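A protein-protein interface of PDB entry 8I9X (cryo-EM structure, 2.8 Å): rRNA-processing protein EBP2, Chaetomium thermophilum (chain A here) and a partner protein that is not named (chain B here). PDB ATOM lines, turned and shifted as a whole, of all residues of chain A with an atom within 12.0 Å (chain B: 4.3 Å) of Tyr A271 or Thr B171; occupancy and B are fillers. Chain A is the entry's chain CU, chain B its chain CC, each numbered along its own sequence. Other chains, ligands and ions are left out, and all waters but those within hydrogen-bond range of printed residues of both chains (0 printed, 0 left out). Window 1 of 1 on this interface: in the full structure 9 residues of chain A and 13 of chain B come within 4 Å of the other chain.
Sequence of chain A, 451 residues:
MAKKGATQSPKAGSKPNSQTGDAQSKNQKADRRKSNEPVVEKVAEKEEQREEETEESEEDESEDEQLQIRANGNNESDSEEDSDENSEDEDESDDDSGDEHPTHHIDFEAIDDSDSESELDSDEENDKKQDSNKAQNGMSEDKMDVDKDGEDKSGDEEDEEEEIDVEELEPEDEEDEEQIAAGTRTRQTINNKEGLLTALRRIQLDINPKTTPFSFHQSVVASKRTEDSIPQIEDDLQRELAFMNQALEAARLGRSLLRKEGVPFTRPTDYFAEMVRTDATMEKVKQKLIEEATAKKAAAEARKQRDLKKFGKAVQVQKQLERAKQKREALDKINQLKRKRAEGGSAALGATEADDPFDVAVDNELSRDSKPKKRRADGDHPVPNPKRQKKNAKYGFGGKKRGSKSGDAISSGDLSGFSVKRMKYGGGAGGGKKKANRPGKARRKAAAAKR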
ATOM      1  N   PRO A 264      31.890 -11.123   8.275  1.00  0.00           N
ATOM      2  CA  PRO A 264      31.032 -12.129   8.910  1.00  0.00           C
ATOM      3  C   PRO A 264      31.849 -13.183   9.639  1.00  0.00           C
ATOM      4  O   PRO A 264      32.870 -13.660   9.140  1.00  0.00           O
ATOM      5  CB  PRO A 264      30.265 -12.725   7.726  1.00  0.00           C
ATOM      6  CG  PRO A 264      30.246 -11.626   6.720  1.00  0.00           C
ATOM      7  CD  PRO A 264      31.593 -10.981   6.840  1.00  0.00           C
ATOM      8  N   PHE A 265      31.393 -13.548  10.837  1.00  0.00           N
ATOM      9  CA  PHE A 265      32.100 -14.500  11.687  1.00  0.00           C
ATOM     10  C   PHE A 265      31.246 -15.731  11.969  1.00  0.00           C
ATOM     11  O   PHE A 265      31.701 -16.857  11.764  1.00  0.00           O
ATOM     12  CB  PHE A 265      32.534 -13.818  12.985  1.00  0.00           C
ATOM     13  CG  PHE A 265      33.571 -14.580  13.756  1.00  0.00           C
ATOM     14  CD1 PHE A 265      33.203 -15.573  14.644  1.00  0.00           C
ATOM     15  CD2 PHE A 265      34.913 -14.299  13.594  1.00  0.00           C
ATOM     16  CE1 PHE A 265      34.155 -16.273  15.353  1.00  0.00           C
ATOM     17  CE2 PHE A 265      35.870 -14.996  14.302  1.00  0.00           C
ATOM     18  CZ  PHE A 265      35.490 -15.984  15.181  1.00  0.00           C
ATOM     19  N   THR A 266      30.016 -15.549  12.443  1.00  0.00           N
ATOM     20  CA  THR A 266      29.195 -16.679  12.851  1.00  0.00           C
ATOM     21  C   THR A 266      28.603 -17.381  11.636  1.00  0.00           C
ATOM     22  O   THR A 266      28.134 -16.740  10.694  1.00  0.00           O
ATOM     23  CB  THR A 266      28.080 -16.204  13.786  1.00  0.00           C
ATOM     24  OG1 THR A 266      28.659 -15.596  14.948  1.00  0.00           O
ATOM     25  CG2 THR A 266      27.212 -17.372  14.227  1.00  0.00           C
ATOM     26  N   ARG A 267      28.630 -18.708  11.664  1.00  0.00           N
ATOM     27  CA  ARG A 267      28.083 -19.498  10.571  1.00  0.00           C
ATOM     28  C   ARG A 267      26.569 -19.591  10.716  1.00  0.00           C
ATOM     29  O   ARG A 267      26.085 -20.050  11.757  1.00  0.00           O
ATOM     30  CB  ARG A 267      28.704 -20.887  10.559  1.00  0.00           C
ATOM     31  CG  ARG A 267      28.328 -21.737   9.360  1.00  0.00           C
ATOM     32  CD  ARG A 267      28.911 -23.129   9.480  1.00  0.00           C
ATOM     33  NE  ARG A 267      28.247 -24.084   8.603  1.00  0.00           N
ATOM     34  CZ  ARG A 267      28.259 -25.397   8.781  1.00  0.00           C
ATOM     35  NH1 ARG A 267      28.890 -25.950   9.803  1.00  0.00           N
ATOM     36  NH2 ARG A 267      27.620 -26.175   7.913  1.00  0.00           N
ATOM     37  N   PRO A 268      25.794 -19.164   9.722  1.00  0.00           N
ATOM     38  CA  PRO A 268      24.334 -19.209   9.852  1.00  0.00           C
ATOM     39  C   PRO A 268      23.821 -20.636   9.952  1.00  0.00           C
ATOM     40  O   PRO A 268      24.425 -21.574   9.427  1.00  0.00           O
ATOM     41  CB  PRO A 268      23.847 -18.526   8.570  1.00  0.00           C
ATOM     42  CG  PRO A 268      24.995 -17.685   8.138  1.00  0.00           C
ATOM     43  CD  PRO A 268      26.206 -18.492   8.482  1.00  0.00           C
ATOM     44  N   THR A 269      22.692 -20.792  10.643  1.00  0.00           N
ATOM     45  CA  THR A 269      22.067 -22.103  10.767  1.00  0.00           C
ATOM     46  C   THR A 269      21.609 -22.644   9.418  1.00  0.00           C
ATOM     47  O   THR A 269      21.551 -23.865   9.235  1.00  0.00           O
ATOM     48  CB  THR A 269      20.890 -22.018  11.742  1.00  0.00           C
ATOM     49  OG1 THR A 269      21.350 -21.483  12.988  1.00  0.00           O
ATOM     50  CG2 THR A 269      20.288 -23.393  11.994  1.00  0.00           C
ATOM     51  N   ASP A 270      21.307 -21.767   8.464  1.00  0.00           N
ATOM     52  CA  ASP A 270      20.843 -22.179   7.149  1.00  0.00           C
ATOM     53  C   ASP A 270      21.963 -22.301   6.122  1.00  0.00           C
ATOM     54  O   ASP A 270      21.674 -22.440   4.929  1.00  0.00           O
ATOM     55  CB  ASP A 270      19.782 -21.197   6.639  1.00  0.00           C
ATOM     56  CG  ASP A 270      20.241 -19.751   6.705  1.00  0.00           C
ATOM     57  OD1 ASP A 270      21.288 -19.422   6.110  1.00  0.00           O
ATOM     58  OD2 ASP A 270      19.550 -18.940   7.354  1.00  0.00           O
ATOM     59  N   TYR A 271      23.225 -22.244   6.545  1.00  0.00           N
ATOM     60  CA  TYR A 271      24.358 -22.409   5.635  1.00  0.00           C
ATOM     61  C   TYR A 271      24.899 -23.826   5.774  1.00  0.00           C
ATOM     62  O   TYR A 271      25.651 -24.129   6.703  1.00  0.00           O
ATOM     63  CB  TYR A 271      25.442 -21.380   5.922  1.00  0.00           C
ATOM     64  CG  TYR A 271      26.646 -21.512   5.018  1.00  0.00           C
ATOM     65  CD1 TYR A 271      27.930 -21.374   5.517  1.00  0.00           C
ATOM     66  CD2 TYR A 271      26.497 -21.779   3.665  1.00  0.00           C
ATOM     67  CE1 TYR A 271      29.030 -21.498   4.697  1.00  0.00           C
ATOM     68  CE2 TYR A 271      27.591 -21.906   2.839  1.00  0.00           C
ATOM     69  CZ  TYR A 271      28.854 -21.762   3.360  1.00  0.00           C
ATOM     70  OH  TYR A 271      29.949 -21.888   2.540  1.00  0.00           O
ATOM     71  N   PHE A 272      24.525 -24.694   4.838  1.00  0.00           N
ATOM     72  CA  PHE A 272      24.986 -26.077   4.799  1.00  0.00           C
ATOM     73  C   PHE A 272      26.061 -26.172   3.725  1.00  0.00           C
ATOM     74  O   PHE A 272      25.806 -25.856   2.559  1.00  0.00           O
ATOM     75  CB  PHE A 272      23.831 -27.030   4.501  1.00  0.00           C
ATOM     76  CG  PHE A 272      22.570 -26.700   5.237  1.00  0.00           C
ATOM     77  CD1 PHE A 272      22.456 -26.950   6.591  1.00  0.00           C
ATOM     78  CD2 PHE A 272      21.497 -26.136   4.574  1.00  0.00           C
ATOM     79  CE1 PHE A 272      21.296 -26.642   7.269  1.00  0.00           C
ATOM     80  CE2 PHE A 272      20.337 -25.828   5.246  1.00  0.00           C
ATOM     81  CZ  PHE A 272      20.236 -26.082   6.594  1.00  0.00           C
ATOM     82  N   ALA A 273      27.256 -26.608   4.112  1.00  0.00           N
ATOM     83  CA  ALA A 273      28.384 -26.671   3.197  1.00  0.00           C
ATOM     84  C   ALA A 273      29.291 -27.828   3.588  1.00  0.00           C
ATOM     85  O   ALA A 273      29.194 -28.381   4.686  1.00  0.00           O
ATOM     86  CB  ALA A 273      29.166 -25.353   3.176  1.00  0.00           C
ATOM     87  N   GLU A 274      30.177 -28.190   2.664  1.00  0.00           N
ATOM     88  CA  GLU A 274      31.057 -29.331   2.864  1.00  0.00           C
ATOM     89  C   GLU A 274      32.020 -29.080   4.019  1.00  0.00           C
ATOM     90  O   GLU A 274      32.448 -27.951   4.270  1.00  0.00           O
ATOM     91  CB  GLU A 274      31.836 -29.627   1.583  1.00  0.00           C
ATOM     92  CG  GLU A 274      32.595 -30.941   1.604  1.00  0.00           C
ATOM     93  CD  GLU A 274      33.145 -31.318   0.244  1.00  0.00           C
ATOM     94  OE1 GLU A 274      32.963 -30.536  -0.711  1.00  0.00           O
ATOM     95  OE2 GLU A 274      33.763 -32.397   0.130  1.00  0.00           O
ATOM     96  N   MET A 275      32.365 -30.156   4.720  1.00  0.00           N
ATOM     97  CA  MET A 275      33.223 -30.112   5.892  1.00  0.00           C
ATOM     98  C   MET A 275      34.550 -30.787   5.568  1.00  0.00           C
ATOM     99  O   MET A 275      34.672 -31.535   4.593  1.00  0.00           O
ATOM    100  CB  MET A 275      32.559 -30.805   7.089  1.00  0.00           C
ATOM    101  CG  MET A 275      31.283 -30.165   7.599  1.00  0.00           C
ATOM    102  SD  MET A 275      31.592 -28.809   8.742  1.00  0.00           S
ATOM    103  CE  MET A 275      31.145 -27.423   7.722  1.00  0.00           C
ATOM    104  N   VAL A 276      35.555 -30.520   6.398  1.00  0.00           N
ATOM    105  CA  VAL A 276      36.813 -31.247   6.296  1.00  0.00           C
ATOM    106  C   VAL A 276      36.658 -32.689   6.770  1.00  0.00           C
ATOM    107  O   VAL A 276      37.502 -33.535   6.460  1.00  0.00           O
ATOM    108  CB  VAL A 276      37.920 -30.525   7.081  1.00  0.00           C
ATOM    109  CG1 VAL A 276      38.160 -29.144   6.505  1.00  0.00           C
ATOM    110  CG2 VAL A 276      37.560 -30.442   8.553  1.00  0.00           C
ATOM    111  N   ASP A 279      30.043 -36.528   7.153  1.00  0.00           N
ATOM    112  CA  ASP A 279      28.920 -36.878   8.014  1.00  0.00           C
ATOM    113  C   ASP A 279      29.060 -38.287   8.564  1.00  0.00           C
ATOM    114  O   ASP A 279      28.652 -38.552   9.697  1.00  0.00           O
ATOM    115  CB  ASP A 279      27.606 -36.750   7.246  1.00  0.00           C
ATOM    116  CG  ASP A 279      27.083 -35.332   7.215  1.00  0.00           C
ATOM    117  OD1 ASP A 279      27.129 -34.714   6.133  1.00  0.00           O
ATOM    118  OD2 ASP A 279      26.624 -34.838   8.266  1.00  0.00           O
ATOM    119  N   VAL B 169      30.164 -19.955  -8.177  1.00  0.00           N
ATOM    120  CA  VAL B 169      29.819 -18.904  -7.227  1.00  0.00           C
ATOM    121  C   VAL B 169      29.144 -19.454  -5.976  1.00  0.00           C
ATOM    122  O   VAL B 169      29.156 -18.793  -4.931  1.00  0.00           O
ATOM    123  CB  VAL B 169      28.925 -17.864  -7.925  1.00  0.00           C
ATOM    124  CG1 VAL B 169      27.624 -18.498  -8.376  1.00  0.00           C
ATOM    125  CG2 VAL B 169      28.668 -16.657  -7.034  1.00  0.00           C
ATOM    126  N   ASN B 170      28.585 -20.664  -6.043  1.00  0.00           N
ATOM    127  CA  ASN B 170      27.724 -21.157  -4.971  1.00  0.00           C
ATOM    128  C   ASN B 170      28.467 -21.321  -3.652  1.00  0.00           C
ATOM    129  O   ASN B 170      27.841 -21.255  -2.588  1.00  0.00           O
ATOM    130  CB  ASN B 170      27.090 -22.485  -5.378  1.00  0.00           C
ATOM    131  CG  ASN B 170      25.883 -22.835  -4.534  1.00  0.00           C
ATOM    132  OD1 ASN B 170      25.373 -22.005  -3.787  1.00  0.00           O
ATOM    133  ND2 ASN B 170      25.419 -24.073  -4.648  1.00  0.00           N
ATOM    134  N   THR B 171      29.780 -21.554  -3.696  1.00  0.00           N
ATOM    135  CA  THR B 171      30.589 -21.776  -2.493  1.00  0.00           C
ATOM    136  C   THR B 171      29.996 -22.918  -1.664  1.00  0.00           C
ATOM    137  O   THR B 171      30.056 -22.936  -0.434  1.00  0.00           O
ATOM    138  CB  THR B 171      30.728 -20.489  -1.674  1.00  0.00           C
ATOM    139  OG1 THR B 171      31.079 -19.412  -2.550  1.00  0.00           O
ATOM    140  CG2 THR B 171      31.840 -20.614  -0.647  1.00  0.00           C
ATOM    141  N   ILE B 172      29.399 -23.877  -2.360  1.00  0.00           N
ATOM    142  CA  ILE B 172      28.833 -25.076  -1.758  1.00  0.00           C
ATOM    143  C   ILE B 172      29.627 -26.257  -2.288  1.00  0.00           C
ATOM    144  O   ILE B 172      29.825 -26.382  -3.502  1.00  0.00           O
ATOM    145  CB  ILE B 172      27.334 -25.219  -2.085  1.00  0.00           C
ATOM    146  CG1 ILE B 172      26.526 -24.152  -1.348  1.00  0.00           C
ATOM    147  CG2 ILE B 172      26.833 -26.603  -1.730  1.00  0.00           C
ATOM    148  CD1 ILE B 172      26.786 -24.110   0.133  1.00  0.00           C
ATOM    149  N   GLY B 173      30.083 -27.117  -1.387  1.00  0.00           N
ATOM    150  CA  GLY B 173      30.989 -28.173  -1.785  1.00  0.00           C
ATOM    151  C   GLY B 173      30.306 -29.341  -2.461  1.00  0.00           C
ATOM    152  O   GLY B 173      29.428 -29.152  -3.306  1.00  0.00           O
ATOM    153  N   TYR B 180      18.457 -27.094   1.595  1.00  0.00           N
ATOM    154  CA  TYR B 180      17.917 -25.937   0.886  1.00  0.00           C
ATOM    155  C   TYR B 180      16.633 -26.246   0.128  1.00  0.00           C
ATOM    156  O   TYR B 180      16.112 -25.368  -0.568  1.00  0.00           O
ATOM    157  CB  TYR B 180      18.933 -25.324  -0.090  1.00  0.00           C
ATOM    158  CG  TYR B 180      20.266 -24.943   0.503  1.00  0.00           C
ATOM    159  CD1 TYR B 180      20.462 -23.694   1.066  1.00  0.00           C
ATOM    160  CD2 TYR B 180      21.343 -25.815   0.456  1.00  0.00           C
ATOM    161  CE1 TYR B 180      21.681 -23.333   1.594  1.00  0.00           C
ATOM    162  CE2 TYR B 180      22.567 -25.462   0.980  1.00  0.00           C
ATOM    163  CZ  TYR B 180      22.731 -24.218   1.546  1.00  0.00           C
ATOM    164  OH  TYR B 180      23.948 -23.858   2.073  1.00  0.00           O
ATOM    165  N   TYR B 188      25.684 -19.723  -0.107  1.00  0.00           N
ATOM    166  CA  TYR B 188      26.194 -18.397   0.215  1.00  0.00           C
ATOM    167  C   TYR B 188      27.362 -18.082  -0.705  1.00  0.00           C
ATOM    168  O   TYR B 188      28.055 -18.991  -1.163  1.00  0.00           O
ATOM    169  CB  TYR B 188      26.655 -18.322   1.674  1.00  0.00           C
ATOM    170  CG  TYR B 188      25.556 -18.004   2.655  1.00  0.00           C
ATOM    171  CD1 TYR B 188      24.609 -18.957   2.996  1.00  0.00           C
ATOM    172  CD2 TYR B 188      25.470 -16.755   3.247  1.00  0.00           C
ATOM    173  CE1 TYR B 188      23.606 -18.672   3.894  1.00  0.00           C
ATOM    174  CE2 TYR B 188      24.471 -16.462   4.147  1.00  0.00           C
ATOM    175  CZ  TYR B 188      23.542 -17.425   4.467  1.00  0.00           C
ATOM    176  OH  TYR B 188      22.542 -17.136   5.364  1.00  0.00           O
ATOM    177  N   ASP B 189      27.586 -16.800  -0.977  1.00  0.00           N
ATOM    178  CA  ASP B 189      28.706 -16.428  -1.827  1.00  0.00           C
ATOM    179  C   ASP B 189      29.982 -16.286  -0.997  1.00  0.00           C
ATOM    180  O   ASP B 189      30.053 -16.691   0.166  1.00  0.00           O
ATOM    181  CB  ASP B 189      28.406 -15.142  -2.598  1.00  0.00           C
ATOM    182  CG  ASP B 189      27.941 -14.007  -1.706  1.00  0.00           C
ATOM    183  OD1 ASP B 189      28.403 -13.909  -0.550  1.00  0.00           O
ATOM    184  OD2 ASP B 189      27.108 -13.201  -2.169  1.00  0.00           O
ATOM    185  N   ILE B 190      31.009 -15.707  -1.620  1.00  0.00           N
ATOM    186  CA  ILE B 190      32.276 -15.458  -0.945  1.00  0.00           C
ATOM    187  C   ILE B 190      32.121 -14.474   0.204  1.00  0.00           C
ATOM    188  O   ILE B 190      32.706 -14.673   1.273  1.00  0.00           O
ATOM    189  CB  ILE B 190      33.306 -14.933  -1.960  1.00  0.00           C
ATOM    190  CG1 ILE B 190      33.923 -16.077  -2.751  1.00  0.00           C
ATOM    191  CG2 ILE B 190      34.402 -14.136  -1.267  1.00  0.00           C
ATOM    192  CD1 ILE B 190      34.615 -15.601  -3.999  1.00  0.00           C
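O of Thr B171 sits at hydrogen-bond distance from OH of Tyr A271, at 3.2 Å. OD1 of Asp A270 sits at hydrogen-bond distance from OH of Tyr B188. The side-chain hydroxyl (OH) of Tyr B180 lies within hydrogen-bond range of the backbone carbonyl oxygen (O) of Phe A272, at 2.8 Å.
The backbone carbonyl oxygen of Asn B170 lies close to the backbone carbonyl oxygen of Tyr B188 (2.7 Å). The side-chain hydroxyl (OG1) of Thr B171 is in hydrogen-bond range of the backbone carbonyl oxygen (O) of Val B169 (3.1 Å). NH2 of Arg A267 sits at hydrogen-bond distance from O of Tyr A271 (3.1 Å). O of Tyr B188 lies close to OG1 of Thr B171 (3.4 Å).
Pro A268 touches Tyr B188 (CB to OH, 3.7 Å). Asp A270 touches Tyr B180. Tyr A271 touches Ile B172. CD2 of Tyr A271 touches OH of Tyr B180, at 3.7 Å. Tyr A271 touches Tyr B188. Ile B172 touches Phe A272. Glu A274 touches Gly B173 (OE1 to CA, 3.3 Å).
Of chain B, only Thr B171 (3.2 Å), Ile B172 (3.6 Å), Tyr B180 (3.7 Å) and Tyr B188 (3.5 Å) come within 4 Å of Tyr A271. Of chain A, only Tyr A271 comes within 4 Å of Thr B171. No residue of chain A comes within 4 Å of Val B169. No residue of chain A comes within 4 Å of Asn B170. Gly B173 touches just one residue of chain A: Glu A274. Asp B189 touches none of the printed residues of chain A. No residue of chain A comes within 4 Å of Ile B190. Printed residues of chain B within 4 Å of Pro A268: Tyr B188 (3.7 Å). Of the printed residues of chain B, Glu A274 touches Gly B173. Printed residues of chain A within 4 Å of Tyr B180: Asp A270, Tyr A271 and Phe A272. Of the printed residues of chain B, Phe A272 touches Ile B172 and Tyr B180. Of the printed residues of chain B, Asp A270 touches Tyr B180 (3.5 Å) and Tyr B188 (2.7 Å).
Hydrophobic or aromatic side chains of chain A that line the printed part of chain B: Pro A268, Tyr A271 and Phe A272. Along chain A the printed residues that touch a printed residue of chain B span positions 268 to 274. Of the 9 printed residues of chain B, 5 touch a printed residue of chain A. Printed residues of chain B that touch a printed residue of chain A: Thr B171, Ile B172, Gly B173, Tyr B180 and Tyr B188. Among the printed residues, no Asp or Glu carboxylate lies within 4 Å of a Lys or Arg side-chain nitrogen of the other chain.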
